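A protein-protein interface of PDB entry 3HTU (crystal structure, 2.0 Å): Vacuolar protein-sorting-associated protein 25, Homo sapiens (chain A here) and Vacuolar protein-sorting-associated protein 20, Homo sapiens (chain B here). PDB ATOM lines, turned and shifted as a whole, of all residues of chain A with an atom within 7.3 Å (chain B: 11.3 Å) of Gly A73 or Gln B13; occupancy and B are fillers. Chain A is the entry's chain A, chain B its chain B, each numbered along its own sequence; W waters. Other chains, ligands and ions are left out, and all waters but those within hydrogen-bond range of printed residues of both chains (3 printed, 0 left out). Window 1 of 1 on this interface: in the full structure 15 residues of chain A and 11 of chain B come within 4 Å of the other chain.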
ATOM      1  N   VAL A  27      14.094 -19.128 -33.012  1.00  0.00           N
ATOM      2  CA  VAL A  27      13.067 -20.001 -32.419  1.00  0.00           C
ATOM      3  C   VAL A  27      12.311 -19.296 -31.265  1.00  0.00           C
ATOM      4  O   VAL A  27      12.932 -18.795 -30.302  1.00  0.00           O
ATOM      5  CB  VAL A  27      13.710 -21.344 -31.971  1.00  0.00           C
ATOM      6  CG1 VAL A  27      12.689 -22.342 -31.656  1.00  0.00           C
ATOM      7  CG2 VAL A  27      14.550 -21.931 -33.120  1.00  0.00           C
ATOM      8  N   PHE A  28      10.982 -19.254 -31.384  1.00  0.00           N
ATOM      9  CA  PHE A  28      10.113 -18.534 -30.445  1.00  0.00           C
ATOM     10  C   PHE A  28       8.959 -19.442 -30.019  1.00  0.00           C
ATOM     11  O   PHE A  28       8.435 -20.179 -30.831  1.00  0.00           O
ATOM     12  CB  PHE A  28       9.525 -17.269 -31.101  1.00  0.00           C
ATOM     13  CG  PHE A  28      10.537 -16.240 -31.497  1.00  0.00           C
ATOM     14  CD1 PHE A  28      11.115 -16.255 -32.774  1.00  0.00           C
ATOM     15  CD2 PHE A  28      10.906 -15.235 -30.616  1.00  0.00           C
ATOM     16  CE1 PHE A  28      12.032 -15.311 -33.144  1.00  0.00           C
ATOM     17  CE2 PHE A  28      11.830 -14.283 -30.985  1.00  0.00           C
ATOM     18  CZ  PHE A  28      12.390 -14.316 -32.246  1.00  0.00           C
ATOM     19  N   THR A  29       8.562 -19.408 -28.748  1.00  0.00           N
ATOM     20  CA  THR A  29       7.281 -20.002 -28.364  1.00  0.00           C
ATOM     21  C   THR A  29       6.174 -19.108 -28.924  1.00  0.00           C
ATOM     22  O   THR A  29       6.395 -17.934 -29.200  1.00  0.00           O
ATOM     23  CB  THR A  29       7.139 -20.230 -26.814  1.00  0.00           C
ATOM     24  OG1 THR A  29       7.135 -18.973 -26.124  1.00  0.00           O
ATOM     25  CG2 THR A  29       8.301 -21.088 -26.275  1.00  0.00           C
ATOM     26  N   ILE A  68       6.109 -25.369 -34.882  1.00  0.00           N
ATOM     27  CA  ILE A  68       6.269 -26.561 -34.036  1.00  0.00           C
ATOM     28  C   ILE A  68       5.050 -26.726 -33.131  1.00  0.00           C
ATOM     29  O   ILE A  68       4.747 -25.864 -32.283  1.00  0.00           O
ATOM     30  CB  ILE A  68       7.602 -26.573 -33.224  1.00  0.00           C
ATOM     31  CG1 ILE A  68       8.807 -26.426 -34.164  1.00  0.00           C
ATOM     32  CG2 ILE A  68       7.790 -27.881 -32.502  1.00  0.00           C
ATOM     33  CD1 ILE A  68       9.378 -25.023 -34.268  1.00  0.00           C
ATOM     34  N   THR A  69       4.369 -27.852 -33.310  1.00  0.00           N
ATOM     35  CA  THR A  69       3.092 -28.070 -32.651  1.00  0.00           C
ATOM     36  C   THR A  69       3.123 -29.107 -31.538  1.00  0.00           C
ATOM     37  O   THR A  69       2.100 -29.323 -30.877  1.00  0.00           O
ATOM     38  CB  THR A  69       1.972 -28.405 -33.649  1.00  0.00           C
ATOM     39  OG1 THR A  69       2.291 -29.615 -34.336  1.00  0.00           O
ATOM     40  CG2 THR A  69       1.809 -27.284 -34.639  1.00  0.00           C
ATOM     41  N   VAL A  70       4.277 -29.719 -31.286  1.00  0.00           N
ATOM     42  CA  VAL A  70       4.348 -30.703 -30.214  1.00  0.00           C
ATOM     43  C   VAL A  70       4.119 -30.030 -28.857  1.00  0.00           C
ATOM     44  O   VAL A  70       4.639 -28.939 -28.588  1.00  0.00           O
ATOM     45  CB  VAL A  70       5.637 -31.586 -30.236  1.00  0.00           C
ATOM     46  CG1 VAL A  70       5.629 -32.529 -31.453  1.00  0.00           C
ATOM     47  CG2 VAL A  70       6.891 -30.754 -30.207  1.00  0.00           C
ATOM     48  N   SER A  71       3.300 -30.684 -28.036  1.00  0.00           N
ATOM     49  CA  SER A  71       2.845 -30.123 -26.774  1.00  0.00           C
ATOM     50  C   SER A  71       3.962 -29.822 -25.773  1.00  0.00           C
ATOM     51  O   SER A  71       3.804 -28.919 -24.941  1.00  0.00           O
ATOM     52  CB  SER A  71       1.822 -31.064 -26.142  1.00  0.00           C
ATOM     53  OG  SER A  71       0.709 -31.223 -26.996  1.00  0.00           O
ATOM     54  N   ASP A  72       5.068 -30.571 -25.855  1.00  0.00           N
ATOM     55  CA  ASP A  72       6.224 -30.409 -24.961  1.00  0.00           C
ATOM     56  C   ASP A  72       7.092 -29.201 -25.289  1.00  0.00           C
ATOM     57  O   ASP A  72       8.066 -28.905 -24.573  1.00  0.00           O
ATOM     58  CB  ASP A  72       7.095 -31.684 -24.917  1.00  0.00           C
ATOM     59  CG  ASP A  72       7.623 -32.099 -26.290  1.00  0.00           C
ATOM     60  OD1 ASP A  72       6.835 -32.152 -27.244  1.00  0.00           O
ATOM     61  OD2 ASP A  72       8.823 -32.407 -26.415  1.00  0.00           O
ATOM     62  N   GLY A  73       6.747 -28.495 -26.358  1.00  0.00           N
ATOM     63  CA  GLY A  73       7.514 -27.335 -26.753  1.00  0.00           C
ATOM     64  C   GLY A  73       7.035 -26.702 -28.034  1.00  0.00           C
ATOM     65  O   GLY A  73       7.706 -26.818 -29.086  1.00  0.00           O
ATOM     66  N   ARG A  74       5.881 -26.034 -27.926  1.00  0.00           N
ATOM     67  CA  ARG A  74       5.178 -25.429 -29.043  1.00  0.00           C
ATOM     68  C   ARG A  74       5.833 -24.125 -29.413  1.00  0.00           C
ATOM     69  O   ARG A  74       6.306 -23.376 -28.542  1.00  0.00           O
ATOM     70  CB  ARG A  74       3.718 -25.111 -28.681  1.00  0.00           C
ATOM     71  CG  ARG A  74       2.802 -26.304 -28.489  1.00  0.00           C
ATOM     72  CD  ARG A  74       1.372 -25.846 -28.163  1.00  0.00           C
ATOM     73  NE  ARG A  74       0.757 -24.982 -29.183  1.00  0.00           N
ATOM     74  CZ  ARG A  74       0.081 -25.427 -30.243  1.00  0.00           C
ATOM     75  NH1 ARG A  74      -0.056 -26.727 -30.447  1.00  0.00           N
ATOM     76  NH2 ARG A  74      -0.452 -24.573 -31.104  1.00  0.00           N
ATOM     77  N   GLY A  75       5.814 -23.820 -30.705  1.00  0.00           N
ATOM     78  CA  GLY A  75       6.363 -22.558 -31.144  1.00  0.00           C
ATOM     79  C   GLY A  75       6.616 -22.514 -32.623  1.00  0.00           C
ATOM     80  O   GLY A  75       5.963 -23.216 -33.390  1.00  0.00           O
ATOM     81  N   VAL A  76       7.567 -21.677 -33.018  1.00  0.00           N
ATOM     82  CA  VAL A  76       7.752 -21.359 -34.413  1.00  0.00           C
ATOM     83  C   VAL A  76       9.230 -21.023 -34.657  1.00  0.00           C
ATOM     84  O   VAL A  76       9.901 -20.423 -33.801  1.00  0.00           O
ATOM     85  CB  VAL A  76       6.747 -20.259 -34.879  1.00  0.00           C
ATOM     86  CG1 VAL A  76       6.934 -18.960 -34.098  1.00  0.00           C
ATOM     87  CG2 VAL A  76       6.839 -19.991 -36.380  1.00  0.00           C
ATOM     88  N   VAL B   4      13.692 -27.783 -38.794  1.00  0.00           N
ATOM     89  CA  VAL B   4      13.774 -27.600 -37.337  1.00  0.00           C
ATOM     90  C   VAL B   4      14.634 -28.701 -36.725  1.00  0.00           C
ATOM     91  O   VAL B   4      14.411 -29.883 -36.997  1.00  0.00           O
ATOM     92  CB  VAL B   4      12.351 -27.573 -36.669  1.00  0.00           C
ATOM     93  CG1 VAL B   4      12.479 -27.453 -35.107  1.00  0.00           C
ATOM     94  CG2 VAL B   4      11.525 -26.405 -37.245  1.00  0.00           C
ATOM     95  N   THR B   5      15.634 -28.307 -35.933  1.00  0.00           N
ATOM     96  CA  THR B   5      16.584 -29.236 -35.317  1.00  0.00           C
ATOM     97  C   THR B   5      16.114 -29.756 -33.946  1.00  0.00           C
ATOM     98  O   THR B   5      15.212 -29.185 -33.321  1.00  0.00           O
ATOM     99  CB  THR B   5      17.980 -28.599 -35.172  1.00  0.00           C
ATOM    100  OG1 THR B   5      17.954 -27.568 -34.174  1.00  0.00           O
ATOM    101  CG2 THR B   5      18.445 -27.994 -36.487  1.00  0.00           C
ATOM    102  N   GLU B   6      16.702 -30.862 -33.506  1.00  0.00           N
ATOM    103  CA  GLU B   6      16.498 -31.382 -32.156  1.00  0.00           C
ATOM    104  C   GLU B   6      16.889 -30.334 -31.091  1.00  0.00           C
ATOM    105  O   GLU B   6      16.201 -30.172 -30.066  1.00  0.00           O
ATOM    106  CB  GLU B   6      17.332 -32.640 -32.004  1.00  0.00           C
ATOM    107  CG  GLU B   6      17.182 -33.364 -30.699  1.00  0.00           C
ATOM    108  CD  GLU B   6      18.274 -34.389 -30.518  1.00  0.00           C
ATOM    109  OE1 GLU B   6      19.285 -34.298 -31.244  1.00  0.00           O
ATOM    110  OE2 GLU B   6      18.124 -35.276 -29.657  1.00  0.00           O
ATOM    111  N   GLN B   7      17.986 -29.630 -31.356  1.00  0.00           N
ATOM    112  CA  GLN B   7      18.393 -28.440 -30.613  1.00  0.00           C
ATOM    113  C   GLN B   7      17.333 -27.327 -30.561  1.00  0.00           C
ATOM    114  O   GLN B   7      17.102 -26.743 -29.496  1.00  0.00           O
ATOM    115  CB  GLN B   7      19.672 -27.884 -31.228  1.00  0.00           C
ATOM    116  CG  GLN B   7      20.067 -26.503 -30.761  1.00  0.00           C
ATOM    117  CD  GLN B   7      21.127 -26.541 -29.709  1.00  0.00           C
ATOM    118  OE1 GLN B   7      22.192 -25.936 -29.875  1.00  0.00           O
ATOM    119  NE2 GLN B   7      20.862 -27.255 -28.612  1.00  0.00           N
ATOM    120  N   ASP B   8      16.730 -27.002 -31.707  1.00  0.00           N
ATOM    121  CA  ASP B   8      15.610 -26.045 -31.770  1.00  0.00           C
ATOM    122  C   ASP B   8      14.447 -26.465 -30.872  1.00  0.00           C
ATOM    123  O   ASP B   8      13.850 -25.626 -30.144  1.00  0.00           O
ATOM    124  CB  ASP B   8      15.064 -25.935 -33.207  1.00  0.00           C
ATOM    125  CG  ASP B   8      15.981 -25.195 -34.139  1.00  0.00           C
ATOM    126  OD1 ASP B   8      16.794 -24.381 -33.647  1.00  0.00           O
ATOM    127  OD2 ASP B   8      15.886 -25.438 -35.376  1.00  0.00           O
ATOM    128  N   LYS B   9      14.104 -27.753 -30.939  1.00  0.00           N
ATOM    129  CA  LYS B   9      13.009 -28.286 -30.119  1.00  0.00           C
ATOM    130  C   LYS B   9      13.357 -28.341 -28.626  1.00  0.00           C
ATOM    131  O   LYS B   9      12.487 -28.135 -27.789  1.00  0.00           O
ATOM    132  CB  LYS B   9      12.562 -29.655 -30.608  1.00  0.00           C
ATOM    133  CG  LYS B   9      11.706 -29.604 -31.881  1.00  0.00           C
ATOM    134  CD  LYS B   9      11.475 -31.004 -32.433  1.00  0.00           C
ATOM    135  CE  LYS B   9      10.665 -30.936 -33.722  1.00  0.00           C
ATOM    136  NZ  LYS B   9      10.920 -32.119 -34.592  1.00  0.00           N
ATOM    137  N   ALA B  10      14.614 -28.638 -28.311  1.00  0.00           N
ATOM    138  CA  ALA B  10      15.116 -28.578 -26.938  1.00  0.00           C
ATOM    139  C   ALA B  10      15.068 -27.162 -26.331  1.00  0.00           C
ATOM    140  O   ALA B  10      14.746 -27.028 -25.156  1.00  0.00           O
ATOM    141  CB  ALA B  10      16.523 -29.170 -26.842  1.00  0.00           C
ATOM    142  N   ILE B  11      15.363 -26.124 -27.122  1.00  0.00           N
ATOM    143  CA  ILE B  11      15.239 -24.738 -26.657  1.00  0.00           C
ATOM    144  C   ILE B  11      13.796 -24.542 -26.256  1.00  0.00           C
ATOM    145  O   ILE B  11      13.479 -24.080 -25.129  1.00  0.00           O
ATOM    146  CB  ILE B  11      15.514 -23.663 -27.765  1.00  0.00           C
ATOM    147  CG1 ILE B  11      16.896 -23.782 -28.421  1.00  0.00           C
ATOM    148  CG2 ILE B  11      15.336 -22.291 -27.231  1.00  0.00           C
ATOM    149  CD1 ILE B  11      18.035 -23.980 -27.515  1.00  0.00           C
ATOM    150  N   LEU B  12      12.930 -24.885 -27.205  1.00  0.00           N
ATOM    151  CA  LEU B  12      11.496 -24.670 -27.075  1.00  0.00           C
ATOM    152  C   LEU B  12      10.823 -25.388 -25.902  1.00  0.00           C
ATOM    153  O   LEU B  12       9.873 -24.859 -25.354  1.00  0.00           O
ATOM    154  CB  LEU B  12      10.789 -25.047 -28.380  1.00  0.00           C
ATOM    155  CG  LEU B  12      10.850 -24.056 -29.534  1.00  0.00           C
ATOM    156  CD1 LEU B  12      10.095 -24.631 -30.713  1.00  0.00           C
ATOM    157  CD2 LEU B  12      10.266 -22.709 -29.132  1.00  0.00           C
ATOM    158  N   GLN B  13      11.262 -26.609 -25.573  1.00  0.00           N
ATOM    159  CA  GLN B  13      10.744 -27.321 -24.392  1.00  0.00           C
ATOM    160  C   GLN B  13      11.041 -26.516 -23.140  1.00  0.00           C
ATOM    161  O   GLN B  13      10.172 -26.388 -22.240  1.00  0.00           O
ATOM    162  CB  GLN B  13      11.347 -28.725 -24.243  1.00  0.00           C
ATOM    163  CG  GLN B  13      11.033 -29.719 -25.393  1.00  0.00           C
ATOM    164  CD  GLN B  13      11.961 -30.923 -25.374  1.00  0.00           C
ATOM    165  OE1 GLN B  13      12.730 -31.107 -24.419  1.00  0.00           O
ATOM    166  NE2 GLN B  13      11.913 -31.746 -26.442  1.00  0.00           N
ATOM    167  N   LEU B  14      12.253 -25.957 -23.088  1.00  0.00           N
ATOM    168  CA  LEU B  14      12.680 -25.172 -21.934  1.00  0.00           C
ATOM    169  C   LEU B  14      11.990 -23.803 -21.915  1.00  0.00           C
ATOM    170  O   LEU B  14      11.476 -23.391 -20.886  1.00  0.00           O
ATOM    171  CB  LEU B  14      14.214 -25.077 -21.859  1.00  0.00           C
ATOM    172  CG  LEU B  14      14.946 -26.426 -21.653  1.00  0.00           C
ATOM    173  CD1 LEU B  14      16.413 -26.328 -21.949  1.00  0.00           C
ATOM    174  CD2 LEU B  14      14.773 -27.011 -20.255  1.00  0.00           C
ATOM    175  N   LYS B  15      11.952 -23.118 -23.057  1.00  0.00           N
ATOM    176  CA  LYS B  15      11.225 -21.854 -23.175  1.00  0.00           C
ATOM    177  C   LYS B  15       9.719 -21.984 -22.857  1.00  0.00           C
ATOM    178  O   LYS B  15       9.102 -21.038 -22.376  1.00  0.00           O
ATOM    179  CB  LYS B  15      11.416 -21.242 -24.564  1.00  0.00           C
ATOM    180  CG  LYS B  15      12.760 -20.578 -24.845  1.00  0.00           C
ATOM    181  CD  LYS B  15      12.665 -19.931 -26.250  1.00  0.00           C
ATOM    182  CE  LYS B  15      13.830 -19.002 -26.614  1.00  0.00           C
ATOM    183  NZ  LYS B  15      13.396 -17.999 -27.682  1.00  0.00           N
ATOM    184  N   GLN B  16       9.130 -23.149 -23.118  1.00  0.00           N
ATOM    185  CA  GLN B  16       7.732 -23.384 -22.748  1.00  0.00           C
ATOM    186  C   GLN B  16       7.516 -23.507 -21.226  1.00  0.00           C
ATOM    187  O   GLN B  16       6.535 -22.973 -20.689  1.00  0.00           O
ATOM    188  CB  GLN B  16       7.162 -24.594 -23.471  1.00  0.00           C
ATOM    189  CG  GLN B  16       5.666 -24.853 -23.139  1.00  0.00           C
ATOM    190  CD  GLN B  16       5.094 -25.965 -23.974  1.00  0.00           C
ATOM    191  OE1 GLN B  16       4.935 -25.835 -25.195  1.00  0.00           O
ATOM    192  NE2 GLN B  16       4.825 -27.088 -23.332  1.00  0.00           N
ATOM    193  N   GLN B  17       8.412 -24.227 -20.550  1.00  0.00           N
ATOM    194  CA  GLN B  17       8.347 -24.402 -19.099  1.00  0.00           C
ATOM    195  C   GLN B  17       8.537 -23.071 -18.379  1.00  0.00           C
ATOM    196  O   GLN B  17       7.918 -22.816 -17.334  1.00  0.00           O
ATOM    197  CB  GLN B  17       9.403 -25.402 -18.638  1.00  0.00           C
ATOM    198  CG  GLN B  17       9.085 -26.833 -19.077  1.00  0.00           C
ATOM    199  CD  GLN B  17      10.186 -27.796 -18.733  1.00  0.00           C
ATOM    200  OE1 GLN B  17      10.425 -28.103 -17.566  1.00  0.00           O
ATOM    201  NE2 GLN B  17      10.862 -28.290 -19.753  1.00  0.00           N
ATOM    202  N   ARG B  18       9.407 -22.251 -18.960  1.00  0.00           N
ATOM    203  CA  ARG B  18       9.619 -20.865 -18.574  1.00  0.00           C
ATOM    204  C   ARG B  18       8.361 -20.008 -18.717  1.00  0.00           C
ATOM    205  O   ARG B  18       8.029 -19.187 -17.833  1.00  0.00           O
ATOM    206  CB  ARG B  18      10.724 -20.292 -19.444  1.00  0.00           C
ATOM    207  CG  ARG B  18      10.933 -18.829 -19.299  1.00  0.00           C
ATOM    208  CD  ARG B  18      11.621 -18.278 -20.504  1.00  0.00           C
ATOM    209  NE  ARG B  18      10.718 -18.153 -21.647  1.00  0.00           N
ATOM    210  CZ  ARG B  18      11.116 -17.807 -22.871  1.00  0.00           C
ATOM    211  NH1 ARG B  18      12.398 -17.547 -23.097  1.00  0.00           N
ATOM    212  NH2 ARG B  18      10.237 -17.721 -23.867  1.00  0.00           N
ATOM    213  N   ASP B  19       7.686 -20.173 -19.851  1.00  0.00           N
ATOM    214  CA  ASP B  19       6.513 -19.396 -20.172  1.00  0.00           C
ATOM    215  C   ASP B  19       5.359 -19.648 -19.194  1.00  0.00           C
ATOM    216  O   ASP B  19       4.717 -18.707 -18.754  1.00  0.00           O
ATOM    217  CB  ASP B  19       6.050 -19.680 -21.597  1.00  0.00           C
ATOM    218  CG  ASP B  19       6.905 -18.995 -22.645  1.00  0.00           C
ATOM    219  OD1 ASP B  19       7.748 -18.140 -22.300  1.00  0.00           O
ATOM    220  OD2 ASP B  19       6.710 -19.311 -23.833  1.00  0.00           O
ATOM    221  N   LYS B  20       5.099 -20.917 -18.884  1.00  0.00           N
ATOM    222  CA  LYS B  20       3.973 -21.294 -18.033  1.00  0.00           C
ATOM    223  C   LYS B  20       4.197 -20.813 -16.606  1.00  0.00           C
ATOM    224  O   LYS B  20       3.233 -20.442 -15.922  1.00  0.00           O
ATOM    225  CB  LYS B  20       3.732 -22.805 -18.025  1.00  0.00           C
ATOM    226  CG  LYS B  20       3.492 -23.445 -19.364  1.00  0.00           C
ATOM    227  CD  LYS B  20       2.048 -23.371 -19.791  1.00  0.00           C
ATOM    228  CE  LYS B  20       1.656 -24.651 -20.436  1.00  0.00           C
ATOM    229  NZ  LYS B  20       2.156 -24.686 -21.813  1.00  0.00           N
ATOM    230  N   LEU B  21       5.459 -20.834 -16.164  1.00  0.00           N
ATOM    231  CA  LEU B  21       5.833 -20.247 -14.866  1.00  0.00           C
ATOM    232  C   LEU B  21       5.686 -18.732 -14.864  1.00  0.00           C
ATOM    233  O   LEU B  21       5.202 -18.146 -13.882  1.00  0.00           O
ATOM    234  CB  LEU B  21       7.242 -20.651 -14.434  1.00  0.00           C
ATOM    235  CG  LEU B  21       7.566 -22.141 -14.326  1.00  0.00           C
ATOM    236  CD1 LEU B  21       8.967 -22.291 -13.818  1.00  0.00           C
ATOM    237  CD2 LEU B  21       6.587 -22.928 -13.448  1.00  0.00           C
ATOM    238  N   ARG B  22       6.078 -18.098 -15.965  1.00  0.00           N
ATOM    239  CA  ARG B  22       5.883 -16.655 -16.135  1.00  0.00           C
ATOM    240  C   ARG B  22       4.390 -16.224 -16.016  1.00  0.00           C
ATOM    241  O   ARG B  22       4.093 -15.183 -15.404  1.00  0.00           O
ATOM    242  CB  ARG B  22       6.494 -16.194 -17.467  1.00  0.00           C
ATOM    243  CG  ARG B  22       7.041 -14.764 -17.451  1.00  0.00           C
ATOM    244  CD  ARG B  22       8.149 -14.602 -18.500  1.00  0.00           C
ATOM    245  NE  ARG B  22       9.421 -15.142 -18.006  1.00  0.00           N
ATOM    246  CZ  ARG B  22      10.609 -15.017 -18.594  1.00  0.00           C
ATOM    247  NH1 ARG B  22      10.766 -14.358 -19.749  1.00  0.00           N
ATOM    248  NH2 ARG B  22      11.660 -15.562 -18.005  1.00  0.00           N
ATOM    249  N   GLN B  23       3.479 -17.012 -16.596  1.00  0.00           N
ATOM    250  CA  GLN B  23       2.019 -16.783 -16.491  1.00  0.00           C
ATOM    251  C   GLN B  23       1.546 -16.820 -15.015  1.00  0.00           C
ATOM    252  O   GLN B  23       0.798 -15.942 -14.564  1.00  0.00           O
ATOM    253  CB  GLN B  23       1.242 -17.836 -17.301  1.00  0.00           C
ATOM    254  CG  GLN B  23       1.487 -17.772 -18.793  1.00  0.00           C
ATOM    255  CD  GLN B  23       1.209 -19.088 -19.523  1.00  0.00           C
ATOM    256  OE1 GLN B  23       0.404 -19.913 -19.083  1.00  0.00           O
ATOM    257  NE2 GLN B  23       1.864 -19.269 -20.657  1.00  0.00           N
HETATM  258  O   HOH W   1       5.326 -23.383 -25.952  1.00  0.00           O
HETATM  259  O   HOH W   2       9.761 -28.569 -29.003  1.00  0.00           O
HETATM  260  O   HOH W   3       9.948 -31.308 -28.556  1.00  0.00           O
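O of Val A27 lies within hydrogen-bond range of NZ of Lys B15 (2.8 Å). The side-chain amide oxygen of Gln B16 lies close to the backbone NH of Gly A73 (3.4 Å). The side-chain amide oxygen (OE1) of Gln B16 is in hydrogen-bond range of the backbone NH (N) of Arg A74, at 2.9 Å. The side-chain hydroxyl of Thr A29 lies close to the side-chain carboxylate of Asp B19, at 2.4 Å. O of Ser A71 sits at hydrogen-bond distance from NE2 of Gln B16 (2.6 Å). The side-chain carboxylate (OD2) of Asp A72 lies within hydrogen-bond range of the side-chain amide nitrogen (NE2) of Gln B13, 3.2 Å away.
O of Thr A69 is in hydrogen-bond range of NH1 of Arg A74, at 3.4 Å. OD1 of Asp B19 is in salt-bridge range of NH2 of Arg B18 (3.0 Å). The backbone NH (N) of Ile A68 lies within hydrogen-bond range of the backbone carbonyl oxygen (O) of Gly A75 (2.6 Å). The backbone NH (N) of Val A76 is in hydrogen-bond range of the backbone carbonyl oxygen (O) of Phe A28, 2.8 Å away. O of Gln B13 is in hydrogen-bond range of NE2 of Gln B17, 3.2 Å away. The guanidinium group (NE) of Arg B18 lies within hydrogen-bond range of the backbone carbonyl oxygen (O) of Lys B15 (3.4 Å).
Among the printed residues, pairs that only touch across the chains: Val A27 with Leu B12 (3.3 Å), Val A27 with Asp B8 (3.4 Å), Phe A28 with Leu B12 (3.6 Å), Thr A29 with Lys B15 (3.6 Å), Gly A73 with Leu B12 (3.6 Å), Ile A68 with Leu B12 (3.6 Å), Asp A72 with Gln B16 (3.7 Å), Thr A29 with Leu B12 (3.7 Å), Thr A29 with Gln B16 (3.9 Å), Ile A68 with Val B4 (3.9 Å) and Gly A73 with Gln B13 (3.996 Å).
Of the printed residues of chain B, Val A27 touches Asp B8, Leu B12 and Lys B15. Of the printed residues of chain B, Phe A28 touches Leu B12. Ile A68 touches just these residues of chain B: Val B4 (3.9 Å) and Leu B12 (3.6 Å). Printed residues of chain B within 4 Å of Asp A72: Gln B13 (3.1 Å) and Gln B16 (3.7 Å). Of the printed residues of chain B, Gly A73 touches Leu B12, Gln B13 and Gln B16. Of the printed residues of chain B, Arg A74 touches Gln B16 (2.9 Å). No residue of chain B comes within 4 Å of Gly A75. Printed residues of chain A within 4 Å of Val B4: Ile A68. Printed residues of chain A within 4 Å of Gln B13: Asp A72 and Gly A73. Of the printed residues of chain A, Gln B16 touches Thr A29, Ser A71, Asp A72, Gly A73 and Arg A74. The nearest printed residue of chain B that does not touch Gly A73 is Lys B9 (5.1 Å).
Hydrophobic or aromatic side chains of chain B within 4 Å of the printed part of chain A: Val B4 and Leu B12. Hydrophobic or aromatic side chains of chain A within 4 Å of the printed part of chain B: Val A27 and Ile A68. Among the printed residues, 17 pairs touch across the chains. Among the printed residues, no Asp or Glu carboxylate lies within 4 Å of a Lys or Arg side-chain nitrogen of the other chain.
Water W1 bridges OE1 of Gln B16 (2.6 Å) and O of Arg A74 (2.8 Å). Water W3 lies within hydrogen-bond range of the side-chain carboxylate (OD2) of Asp A72 (2.7 Å) and the side-chain amide nitrogen (NE2) of Gln B13 (2.9 Å). Water W2 bridges the backbone carbonyl oxygen of Gly A73 (2.7 Å) and the backbone carbonyl oxygen of Lys B9 (3.0 Å).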
